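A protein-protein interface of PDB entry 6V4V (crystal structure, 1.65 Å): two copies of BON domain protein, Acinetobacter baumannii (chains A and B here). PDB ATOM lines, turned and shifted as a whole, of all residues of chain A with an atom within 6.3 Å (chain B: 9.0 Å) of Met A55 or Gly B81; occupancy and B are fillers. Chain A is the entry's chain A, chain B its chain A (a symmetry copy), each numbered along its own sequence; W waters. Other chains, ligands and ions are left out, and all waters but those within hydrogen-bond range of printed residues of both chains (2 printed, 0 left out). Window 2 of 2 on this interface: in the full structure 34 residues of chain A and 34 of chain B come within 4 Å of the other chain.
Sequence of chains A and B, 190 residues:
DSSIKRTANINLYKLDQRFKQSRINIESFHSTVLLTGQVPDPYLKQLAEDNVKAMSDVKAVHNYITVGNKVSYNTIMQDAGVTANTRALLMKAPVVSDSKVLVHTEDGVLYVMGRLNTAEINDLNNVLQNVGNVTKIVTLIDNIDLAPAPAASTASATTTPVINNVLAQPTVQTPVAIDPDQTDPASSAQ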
ATOM      1  N   ILE A  26      27.418  -9.519 -20.900  1.00  0.00           N
ATOM      2  CA  ILE A  26      27.598  -8.163 -21.415  1.00  0.00           C
ATOM      3  C   ILE A  26      28.949  -7.698 -20.915  1.00  0.00           C
ATOM      4  O   ILE A  26      29.123  -7.488 -19.707  1.00  0.00           O
ATOM      5  CB  ILE A  26      26.488  -7.217 -20.933  1.00  0.00           C
ATOM      6  CG1 ILE A  26      25.111  -7.815 -21.211  1.00  0.00           C
ATOM      7  CG2 ILE A  26      26.641  -5.823 -21.536  1.00  0.00           C
ATOM      8  CD1 ILE A  26      23.987  -7.082 -20.496  1.00  0.00           C
ATOM      9  N   VAL A  33      31.008  -2.813 -26.626  1.00  0.00           N
ATOM     10  CA  VAL A  33      30.394  -3.895 -25.858  1.00  0.00           C
ATOM     11  C   VAL A  33      30.385  -5.176 -26.680  1.00  0.00           C
ATOM     12  O   VAL A  33      30.027  -5.174 -27.867  1.00  0.00           O
ATOM     13  CB  VAL A  33      28.969  -3.541 -25.387  1.00  0.00           C
ATOM     14  CG1 VAL A  33      28.423  -4.657 -24.488  1.00  0.00           C
ATOM     15  CG2 VAL A  33      28.977  -2.227 -24.620  1.00  0.00           C
ATOM     16  N   ASP A  50      19.419  -3.904 -28.550  1.00  0.00           N
ATOM     17  CA  ASP A  50      18.782  -2.584 -28.493  1.00  0.00           C
ATOM     18  C   ASP A  50      18.989  -1.926 -27.135  1.00  0.00           C
ATOM     19  O   ASP A  50      19.320  -0.732 -27.054  1.00  0.00           O
ATOM     20  CB  ASP A  50      17.278  -2.681 -28.782  1.00  0.00           C
ATOM     21  CG  ASP A  50      16.960  -3.077 -30.229  1.00  0.00           C
ATOM     22  OD1 ASP A  50      17.831  -2.969 -31.110  1.00  0.00           O
ATOM     23  OD2 ASP A  50      15.811  -3.468 -30.486  1.00  0.00           O
ATOM     24  N   ASN A  51      18.797  -2.685 -26.057  1.00  0.00           N
ATOM     25  CA  ASN A  51      18.944  -2.118 -24.717  1.00  0.00           C
ATOM     26  C   ASN A  51      20.387  -1.710 -24.425  1.00  0.00           C
ATOM     27  O   ASN A  51      20.630  -0.693 -23.762  1.00  0.00           O
ATOM     28  CB  ASN A  51      18.462  -3.122 -23.665  1.00  0.00           C
ATOM     29  CG  ASN A  51      16.956  -3.337 -23.692  1.00  0.00           C
ATOM     30  OD1 ASN A  51      16.191  -2.504 -24.209  1.00  0.00           O
ATOM     31  ND2 ASN A  51      16.521  -4.457 -23.146  1.00  0.00           N
ATOM     32  N   VAL A  52      21.362  -2.499 -24.872  1.00  0.00           N
ATOM     33  CA  VAL A  52      22.754  -2.124 -24.638  1.00  0.00           C
ATOM     34  C   VAL A  52      23.139  -0.911 -25.482  1.00  0.00           C
ATOM     35  O   VAL A  52      23.836   0.000 -25.013  1.00  0.00           O
ATOM     36  CB  VAL A  52      23.674  -3.324 -24.916  1.00  0.00           C
ATOM     37  CG1 VAL A  52      25.112  -2.870 -25.005  1.00  0.00           C
ATOM     38  CG2 VAL A  52      23.502  -4.398 -23.835  1.00  0.00           C
ATOM     39  N   LYS A  53      22.677  -0.865 -26.739  1.00  0.00           N
ATOM     40  CA  LYS A  53      22.998   0.278 -27.584  1.00  0.00           C
ATOM     41  C   LYS A  53      22.432   1.576 -27.029  1.00  0.00           C
ATOM     42  O   LYS A  53      22.942   2.652 -27.358  1.00  0.00           O
ATOM     43  CB  LYS A  53      22.461   0.072 -29.003  1.00  0.00           C
ATOM     44  CG  LYS A  53      23.206  -0.936 -29.861  1.00  0.00           C
ATOM     45  CD  LYS A  53      22.897  -0.653 -31.338  1.00  0.00           C
ATOM     46  CE  LYS A  53      22.675  -1.907 -32.153  1.00  0.00           C
ATOM     47  NZ  LYS A  53      23.696  -2.122 -33.230  1.00  0.00           N
ATOM     48  N   ALA A  54      21.378   1.502 -26.219  1.00  0.00           N
ATOM     49  CA  ALA A  54      20.734   2.699 -25.691  1.00  0.00           C
ATOM     50  C   ALA A  54      21.447   3.256 -24.471  1.00  0.00           C
ATOM     51  O   ALA A  54      21.111   4.360 -24.031  1.00  0.00           O
ATOM     52  CB  ALA A  54      19.275   2.406 -25.335  1.00  0.00           C
ATOM     53  N   MET A  55      22.411   2.528 -23.919  1.00  0.00           N
ATOM     54  CA  MET A  55      23.113   2.987 -22.737  1.00  0.00           C
ATOM     55  C   MET A  55      24.015   4.152 -23.080  1.00  0.00           C
ATOM     56  O   MET A  55      24.658   4.173 -24.132  1.00  0.00           O
ATOM     57  CB  MET A  55      23.926   1.854 -22.110  1.00  0.00           C
ATOM     58  CG  MET A  55      23.103   0.628 -21.852  1.00  0.00           C
ATOM     59  SD  MET A  55      24.034  -0.843 -20.961  1.00  0.00           S
ATOM     60  CE  MET A  55      25.618  -1.018 -22.036  1.00  0.00           C
ATOM     61  N   SER A  56      24.039   5.136 -22.188  1.00  0.00           N
ATOM     62  CA  SER A  56      24.989   6.227 -22.319  1.00  0.00           C
ATOM     63  C   SER A  56      26.399   5.669 -22.448  1.00  0.00           C
ATOM     64  O   SER A  56      26.750   4.674 -21.809  1.00  0.00           O
ATOM     65  CB  SER A  56      24.900   7.153 -21.105  1.00  0.00           C
ATOM     66  OG  SER A  56      25.346   6.484 -19.936  1.00  0.00           O
ATOM     67  N   ASP A  57      27.195   6.301 -23.307  1.00  0.00           N
ATOM     68  CA  ASP A  57      28.629   6.074 -23.451  1.00  0.00           C
ATOM     69  C   ASP A  57      28.969   4.780 -24.180  1.00  0.00           C
ATOM     70  O   ASP A  57      30.138   4.379 -24.187  1.00  0.00           O
ATOM     71  CB  ASP A  57      29.344   6.093 -22.091  1.00  0.00           C
ATOM     72  CG  ASP A  57      28.751   7.114 -21.123  1.00  0.00           C
ATOM     73  OD1 ASP A  57      28.835   8.331 -21.403  1.00  0.00           O
ATOM     74  OD2 ASP A  57      28.182   6.686 -20.090  1.00  0.00           O
ATOM     75  N   VAL A  58      27.996   4.116 -24.803  1.00  0.00           N
ATOM     76  CA  VAL A  58      28.246   2.912 -25.586  1.00  0.00           C
ATOM     77  C   VAL A  58      28.350   3.309 -27.051  1.00  0.00           C
ATOM     78  O   VAL A  58      27.414   3.897 -27.607  1.00  0.00           O
ATOM     79  CB  VAL A  58      27.140   1.866 -25.380  1.00  0.00           C
ATOM     80  CG1 VAL A  58      27.310   0.727 -26.373  1.00  0.00           C
ATOM     81  CG2 VAL A  58      27.173   1.341 -23.957  1.00  0.00           C
ATOM     82  N   LYS A  59      29.485   2.994 -27.683  1.00  0.00           N
ATOM     83  CA  LYS A  59      29.742   3.419 -29.059  1.00  0.00           C
ATOM     84  C   LYS A  59      29.419   2.340 -30.083  1.00  0.00           C
ATOM     85  O   LYS A  59      28.768   2.617 -31.093  1.00  0.00           O
ATOM     86  CB  LYS A  59      31.207   3.847 -29.229  1.00  0.00           C
ATOM     87  CG  LYS A  59      31.520   5.249 -28.756  1.00  0.00           C
ATOM     88  CD  LYS A  59      33.020   5.499 -28.760  1.00  0.00           C
ATOM     89  CE  LYS A  59      33.386   6.694 -27.896  1.00  0.00           C
ATOM     90  NZ  LYS A  59      34.614   6.435 -27.091  1.00  0.00           N
ATOM     91  N   ASN B  74      15.835  -7.120 -16.361  1.00  0.00           N
ATOM     92  CA  ASN B  74      15.997  -5.697 -16.097  1.00  0.00           C
ATOM     93  C   ASN B  74      17.167  -5.429 -15.152  1.00  0.00           C
ATOM     94  O   ASN B  74      17.845  -4.405 -15.286  1.00  0.00           O
ATOM     95  CB  ASN B  74      14.707  -5.108 -15.531  1.00  0.00           C
ATOM     96  CG  ASN B  74      13.637  -4.926 -16.594  1.00  0.00           C
ATOM     97  OD1 ASN B  74      13.933  -4.870 -17.792  1.00  0.00           O
ATOM     98  ND2 ASN B  74      12.387  -4.813 -16.159  1.00  0.00           N
ATOM     99  N   THR B  75      17.432  -6.332 -14.200  1.00  0.00           N
ATOM    100  CA  THR B  75      18.571  -6.127 -13.317  1.00  0.00           C
ATOM    101  C   THR B  75      19.898  -6.222 -14.071  1.00  0.00           C
ATOM    102  O   THR B  75      20.781  -5.381 -13.875  1.00  0.00           O
ATOM    103  CB  THR B  75      18.529  -7.129 -12.161  1.00  0.00           C
ATOM    104  OG1 THR B  75      17.383  -6.839 -11.338  1.00  0.00           O
ATOM    105  CG2 THR B  75      19.812  -7.018 -11.327  1.00  0.00           C
ATOM    106  N   ILE B  76      20.070  -7.220 -14.947  1.00  0.00           N
ATOM    107  CA  ILE B  76      21.366  -7.274 -15.629  1.00  0.00           C
ATOM    108  C   ILE B  76      21.551  -6.072 -16.557  1.00  0.00           C
ATOM    109  O   ILE B  76      22.681  -5.609 -16.761  1.00  0.00           O
ATOM    110  CB  ILE B  76      21.590  -8.612 -16.374  1.00  0.00           C
ATOM    111  CG1 ILE B  76      20.796  -8.709 -17.672  1.00  0.00           C
ATOM    112  CG2 ILE B  76      21.355  -9.831 -15.433  1.00  0.00           C
ATOM    113  CD1 ILE B  76      21.415  -9.684 -18.653  1.00  0.00           C
ATOM    114  N   MET B  77      20.473  -5.534 -17.124  1.00  0.00           N
ATOM    115  CA  MET B  77      20.601  -4.341 -17.962  1.00  0.00           C
ATOM    116  C   MET B  77      20.910  -3.091 -17.130  1.00  0.00           C
ATOM    117  O   MET B  77      21.663  -2.218 -17.558  1.00  0.00           O
ATOM    118  CB  MET B  77      19.333  -4.129 -18.786  1.00  0.00           C
ATOM    119  CG  MET B  77      19.185  -5.185 -19.882  1.00  0.00           C
ATOM    120  SD  MET B  77      20.704  -5.075 -21.134  1.00  0.00           S
ATOM    121  CE  MET B  77      20.649  -6.906 -21.838  1.00  0.00           C
ATOM    122  N   GLN B  78      20.311  -2.991 -15.943  1.00  0.00           N
ATOM    123  CA  GLN B  78      20.670  -1.889 -15.062  1.00  0.00           C
ATOM    124  C   GLN B  78      22.122  -2.009 -14.632  1.00  0.00           C
ATOM    125  O   GLN B  78      22.865  -1.024 -14.658  1.00  0.00           O
ATOM    126  CB  GLN B  78      19.755  -1.845 -13.845  1.00  0.00           C
ATOM    127  CG  GLN B  78      20.093  -0.693 -12.905  1.00  0.00           C
ATOM    128  CD  GLN B  78      19.044  -0.499 -11.839  1.00  0.00           C
ATOM    129  OE1 GLN B  78      18.865  -1.348 -10.965  1.00  0.00           O
ATOM    130  NE2 GLN B  78      18.317   0.609 -11.921  1.00  0.00           N
ATOM    131  N   ASP B  79      22.542  -3.220 -14.258  1.00  0.00           N
ATOM    132  CA  ASP B  79      23.937  -3.487 -13.906  1.00  0.00           C
ATOM    133  C   ASP B  79      24.885  -3.052 -15.023  1.00  0.00           C
ATOM    134  O   ASP B  79      25.886  -2.368 -14.773  1.00  0.00           O
ATOM    135  CB  ASP B  79      24.120  -4.977 -13.631  1.00  0.00           C
ATOM    136  CG  ASP B  79      23.496  -5.436 -12.313  1.00  0.00           C
ATOM    137  OD1 ASP B  79      23.164  -4.605 -11.441  1.00  0.00           O
ATOM    138  OD2 ASP B  79      23.345  -6.668 -12.168  1.00  0.00           O
ATOM    139  N   ALA B  80      24.597  -3.470 -16.269  1.00  0.00           N
ATOM    140  CA  ALA B  80      25.456  -3.082 -17.385  1.00  0.00           C
ATOM    141  C   ALA B  80      25.536  -1.569 -17.525  1.00  0.00           C
ATOM    142  O   ALA B  80      26.587  -1.028 -17.894  1.00  0.00           O
ATOM    143  CB  ALA B  80      24.958  -3.731 -18.690  1.00  0.00           C
ATOM    144  N   GLY B  81      24.435  -0.863 -17.259  1.00  0.00           N
ATOM    145  CA  GLY B  81      24.453   0.586 -17.379  1.00  0.00           C
ATOM    146  C   GLY B  81      25.302   1.240 -16.310  1.00  0.00           C
ATOM    147  O   GLY B  81      25.952   2.255 -16.561  1.00  0.00           O
ATOM    148  N   VAL B  82      25.318   0.657 -15.112  1.00  0.00           N
ATOM    149  CA  VAL B  82      26.220   1.131 -14.063  1.00  0.00           C
ATOM    150  C   VAL B  82      27.669   0.950 -14.494  1.00  0.00           C
ATOM    151  O   VAL B  82      28.497   1.857 -14.367  1.00  0.00           O
ATOM    152  CB  VAL B  82      25.935   0.395 -12.745  1.00  0.00           C
ATOM    153  CG1 VAL B  82      27.092   0.632 -11.761  1.00  0.00           C
ATOM    154  CG2 VAL B  82      24.602   0.853 -12.150  1.00  0.00           C
ATOM    155  N   THR B  83      27.994  -0.233 -15.009  1.00  0.00           N
ATOM    156  CA  THR B  83      29.338  -0.474 -15.517  1.00  0.00           C
ATOM    157  C   THR B  83      29.700   0.505 -16.630  1.00  0.00           C
ATOM    158  O   THR B  83      30.788   1.092 -16.621  1.00  0.00           O
ATOM    159  CB  THR B  83      29.451  -1.916 -15.995  1.00  0.00           C
ATOM    160  OG1 THR B  83      29.305  -2.786 -14.867  1.00  0.00           O
ATOM    161  CG2 THR B  83      30.800  -2.151 -16.669  1.00  0.00           C
ATOM    162  N   ALA B  84      28.789   0.721 -17.591  1.00  0.00           N
ATOM    163  CA  ALA B  84      29.068   1.672 -18.667  1.00  0.00           C
ATOM    164  C   ALA B  84      29.283   3.087 -18.133  1.00  0.00           C
ATOM    165  O   ALA B  84      30.161   3.814 -18.611  1.00  0.00           O
ATOM    166  CB  ALA B  84      27.932   1.668 -19.693  1.00  0.00           C
ATOM    167  N   ASN B  85      28.486   3.497 -17.145  1.00  0.00           N
ATOM    168  CA  ASN B  85      28.677   4.806 -16.536  1.00  0.00           C
ATOM    169  C   ASN B  85      30.031   4.893 -15.838  1.00  0.00           C
ATOM    170  O   ASN B  85      30.706   5.930 -15.903  1.00  0.00           O
ATOM    171  CB  ASN B  85      27.532   5.091 -15.563  1.00  0.00           C
ATOM    172  CG  ASN B  85      27.740   6.372 -14.758  1.00  0.00           C
ATOM    173  OD1 ASN B  85      28.346   7.331 -15.241  1.00  0.00           O
ATOM    174  ND2 ASN B  85      27.212   6.400 -13.536  1.00  0.00           N
ATOM    175  N   THR B  86      30.457   3.808 -15.188  1.00  0.00           N
ATOM    176  CA  THR B  86      31.739   3.826 -14.491  1.00  0.00           C
ATOM    177  C   THR B  86      32.898   3.927 -15.474  1.00  0.00           C
ATOM    178  O   THR B  86      33.839   4.700 -15.259  1.00  0.00           O
ATOM    179  CB  THR B  86      31.878   2.574 -13.628  1.00  0.00           C
ATOM    180  OG1 THR B  86      30.747   2.468 -12.753  1.00  0.00           O
ATOM    181  CG2 THR B  86      33.174   2.633 -12.801  1.00  0.00           C
ATOM    182  N   ARG B  87      32.852   3.145 -16.556  1.00  0.00           N
ATOM    183  CA  ARG B  87      33.901   3.198 -17.568  1.00  0.00           C
ATOM    184  C   ARG B  87      34.030   4.590 -18.171  1.00  0.00           C
ATOM    185  O   ARG B  87      35.144   5.055 -18.430  1.00  0.00           O
ATOM    186  CB  ARG B  87      33.622   2.162 -18.653  1.00  0.00           C
ATOM    187  CG  ARG B  87      33.917   0.749 -18.186  1.00  0.00           C
ATOM    188  CD  ARG B  87      34.575  -0.061 -19.281  1.00  0.00           C
ATOM    189  NE  ARG B  87      35.286  -1.214 -18.738  1.00  0.00           N
ATOM    190  CZ  ARG B  87      36.494  -1.149 -18.190  1.00  0.00           C
ATOM    191  NH1 ARG B  87      37.126   0.015 -18.116  1.00  0.00           N
ATOM    192  NH2 ARG B  87      37.071  -2.245 -17.720  1.00  0.00           N
ATOM    193  N   ALA B  88      32.901   5.267 -18.406  1.00  0.00           N
ATOM    194  CA  ALA B  88      32.954   6.626 -18.941  1.00  0.00           C
ATOM    195  C   ALA B  88      33.639   7.576 -17.967  1.00  0.00           C
ATOM    196  O   ALA B  88      34.465   8.405 -18.370  1.00  0.00           O
ATOM    197  CB  ALA B  88      31.548   7.120 -19.266  1.00  0.00           C
ATOM    198  N   LEU B  89      33.317   7.465 -16.676  1.00  0.00           N
ATOM    199  CA  LEU B  89      33.971   8.312 -15.686  1.00  0.00           C
ATOM    200  C   LEU B  89      35.461   8.003 -15.578  1.00  0.00           C
ATOM    201  O   LEU B  89      36.264   8.909 -15.335  1.00  0.00           O
ATOM    202  CB  LEU B  89      33.289   8.149 -14.327  1.00  0.00           C
ATOM    203  CG  LEU B  89      31.837   8.622 -14.222  1.00  0.00           C
ATOM    204  CD1 LEU B  89      31.233   8.243 -12.879  1.00  0.00           C
ATOM    205  CD2 LEU B  89      31.723  10.128 -14.464  1.00  0.00           C
ATOM    206  N   VAL B 103      35.810  -3.665 -14.561  1.00  0.00           N
ATOM    207  CA  VAL B 103      34.608  -3.211 -13.879  1.00  0.00           C
ATOM    208  C   VAL B 103      33.493  -4.203 -14.162  1.00  0.00           C
ATOM    209  O   VAL B 103      33.246  -4.543 -15.326  1.00  0.00           O
ATOM    210  CB  VAL B 103      34.194  -1.800 -14.339  1.00  0.00           C
ATOM    211  CG1 VAL B 103      32.993  -1.318 -13.531  1.00  0.00           C
ATOM    212  CG2 VAL B 103      35.374  -0.828 -14.217  1.00  0.00           C
ATOM    213  N   THR B 105      29.351  -5.081 -12.592  1.00  0.00           N
ATOM    214  CA  THR B 105      28.263  -4.834 -11.655  1.00  0.00           C
ATOM    215  C   THR B 105      27.342  -6.043 -11.656  1.00  0.00           C
ATOM    216  O   THR B 105      26.914  -6.496 -12.718  1.00  0.00           O
ATOM    217  CB  THR B 105      27.483  -3.566 -12.021  1.00  0.00           C
ATOM    218  OG1 THR B 105      28.394  -2.463 -12.138  1.00  0.00           O
ATOM    219  CG2 THR B 105      26.435  -3.250 -10.952  1.00  0.00           C
ATOM    220  N   LEU B 110      28.960  -2.925  -7.353  1.00  0.00           N
ATOM    221  CA  LEU B 110      29.994  -2.524  -8.297  1.00  0.00           C
ATOM    222  C   LEU B 110      31.327  -3.134  -7.869  1.00  0.00           C
ATOM    223  O   LEU B 110      31.832  -2.830  -6.782  1.00  0.00           O
ATOM    224  CB  LEU B 110      30.082  -0.997  -8.354  1.00  0.00           C
ATOM    225  CG  LEU B 110      31.112  -0.364  -9.286  1.00  0.00           C
ATOM    226  CD1 LEU B 110      30.862  -0.804 -10.702  1.00  0.00           C
ATOM    227  CD2 LEU B 110      31.036   1.146  -9.200  1.00  0.00           C
ATOM    228  N   VAL B 131      29.190   7.277  -8.843  1.00  0.00           N
ATOM    229  CA  VAL B 131      28.437   6.328  -9.656  1.00  0.00           C
ATOM    230  C   VAL B 131      27.091   6.081  -8.989  1.00  0.00           C
ATOM    231  O   VAL B 131      27.029   5.692  -7.818  1.00  0.00           O
ATOM    232  CB  VAL B 131      29.216   5.019  -9.857  1.00  0.00           C
ATOM    233  CG1 VAL B 131      28.404   4.048 -10.697  1.00  0.00           C
ATOM    234  CG2 VAL B 131      30.546   5.307 -10.538  1.00  0.00           C
ATOM    235  N   GLY B 132      26.003   6.323  -9.734  1.00  0.00           N
ATOM    236  CA  GLY B 132      24.671   6.078  -9.224  1.00  0.00           C
ATOM    237  C   GLY B 132      24.211   4.642  -9.418  1.00  0.00           C
ATOM    238  O   GLY B 132      24.810   3.872 -10.171  1.00  0.00           O
ATOM    239  N   ASN B 133      23.127   4.303  -8.710  1.00  0.00           N
ATOM    240  CA  ASN B 133      22.466   2.997  -8.801  1.00  0.00           C
ATOM    241  C   ASN B 133      23.361   1.871  -8.284  1.00  0.00           C
ATOM    242  O   ASN B 133      23.352   0.759  -8.817  1.00  0.00           O
ATOM    243  CB  ASN B 133      21.999   2.697 -10.228  1.00  0.00           C
ATOM    244  CG  ASN B 133      20.878   3.615 -10.684  1.00  0.00           C
ATOM    245  OD1 ASN B 133      20.966   4.242 -11.740  1.00  0.00           O
ATOM    246  ND2 ASN B 133      19.817   3.695  -9.890  1.00  0.00           N
ATOM    247  N   VAL B 134      24.110   2.150  -7.223  1.00  0.00           N
ATOM    248  CA  VAL B 134      25.059   1.208  -6.636  1.00  0.00           C
ATOM    249  C   VAL B 134      24.742   1.085  -5.151  1.00  0.00           C
ATOM    250  O   VAL B 134      24.797   2.083  -4.424  1.00  0.00           O
ATOM    251  CB  VAL B 134      26.512   1.678  -6.831  1.00  0.00           C
ATOM    252  CG1 VAL B 134      27.453   0.856  -5.983  1.00  0.00           C
ATOM    253  CG2 VAL B 134      26.903   1.603  -8.296  1.00  0.00           C
HETATM  254  O   HOH W   1      24.583   3.622 -18.963  1.00  0.00           O
HETATM  255  O   HOH W   2      31.023   3.465 -21.309  1.00  0.00           O
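The backbone NH (N) of Gly B81 sits at hydrogen-bond distance from the side-chain sulfur (SD) of Met A55 (3.7 Å).
OG of Ser A56 is in hydrogen-bond range of OD2 of Asp A57 (2.8 Å).
Among the printed residues, pairs that only touch across the chains: Ile A26 with Met B77, Ile A26 with Ala B80, Asn A51 with Met B77, Val A52 with Met B77, Met A55 with Ala B80, Ser A56 with Ala B84, Asp A57 with Ala B84 and Asp A57 with Ala B88.
Printed residues of chain B within 4 Å of Ile A26: Met B77 and Ala B80.
Val A52 touches just one residue of chain B: Met B77.
Lys A53 touches none of the printed residues of chain B.
No residue of chain B comes within 4 Å of Ala A54.
Of chain B, only Ala B80 (3.8 Å) and Gly B81 (3.7 Å) come within 4 Å of Met A55.
Ser A56 touches just one residue of chain B: Ala B84.
Printed residues of chain B within 4 Å of Asp A57: Ala B84 and Ala B88.
No residue of chain B comes within 4 Å of Val A58.
Of chain A, only Met A55 comes within 4 Å of Gly B81.
Leu B89 touches none of the printed residues of chain A.
The nearest residue of chain A that does not touch Gly B81 is Ser A56 (5.4 Å).
Of the 23 printed residues of chain B, 5 touch a printed residue of chain A.
Printed residues of chain A that touch a printed residue of chain B: Ile A26, Asn A51, Val A52, Met A55, Ser A56 and Asp A57.
Hydrophobic or aromatic side chains of chain A within 4 Å of the printed part of chain B: Ile A26, Val A52 and Met A55.
Among the printed residues, 9 pairs touch across the chains.
Among the printed residues, no Asp or Glu carboxylate lies within 4 Å of a Lys or Arg side-chain nitrogen of the other chain.
No position is printed for both chains.
Water W2 bridges the backbone carbonyl oxygen (O) of Ala B84 and the backbone carbonyl oxygen (O) of Asp A57.
Water W1 bridges the backbone carbonyl oxygen of Gly B81 (3.1 Å) and the side-chain hydroxyl of Ser A56 (3.1 Å).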
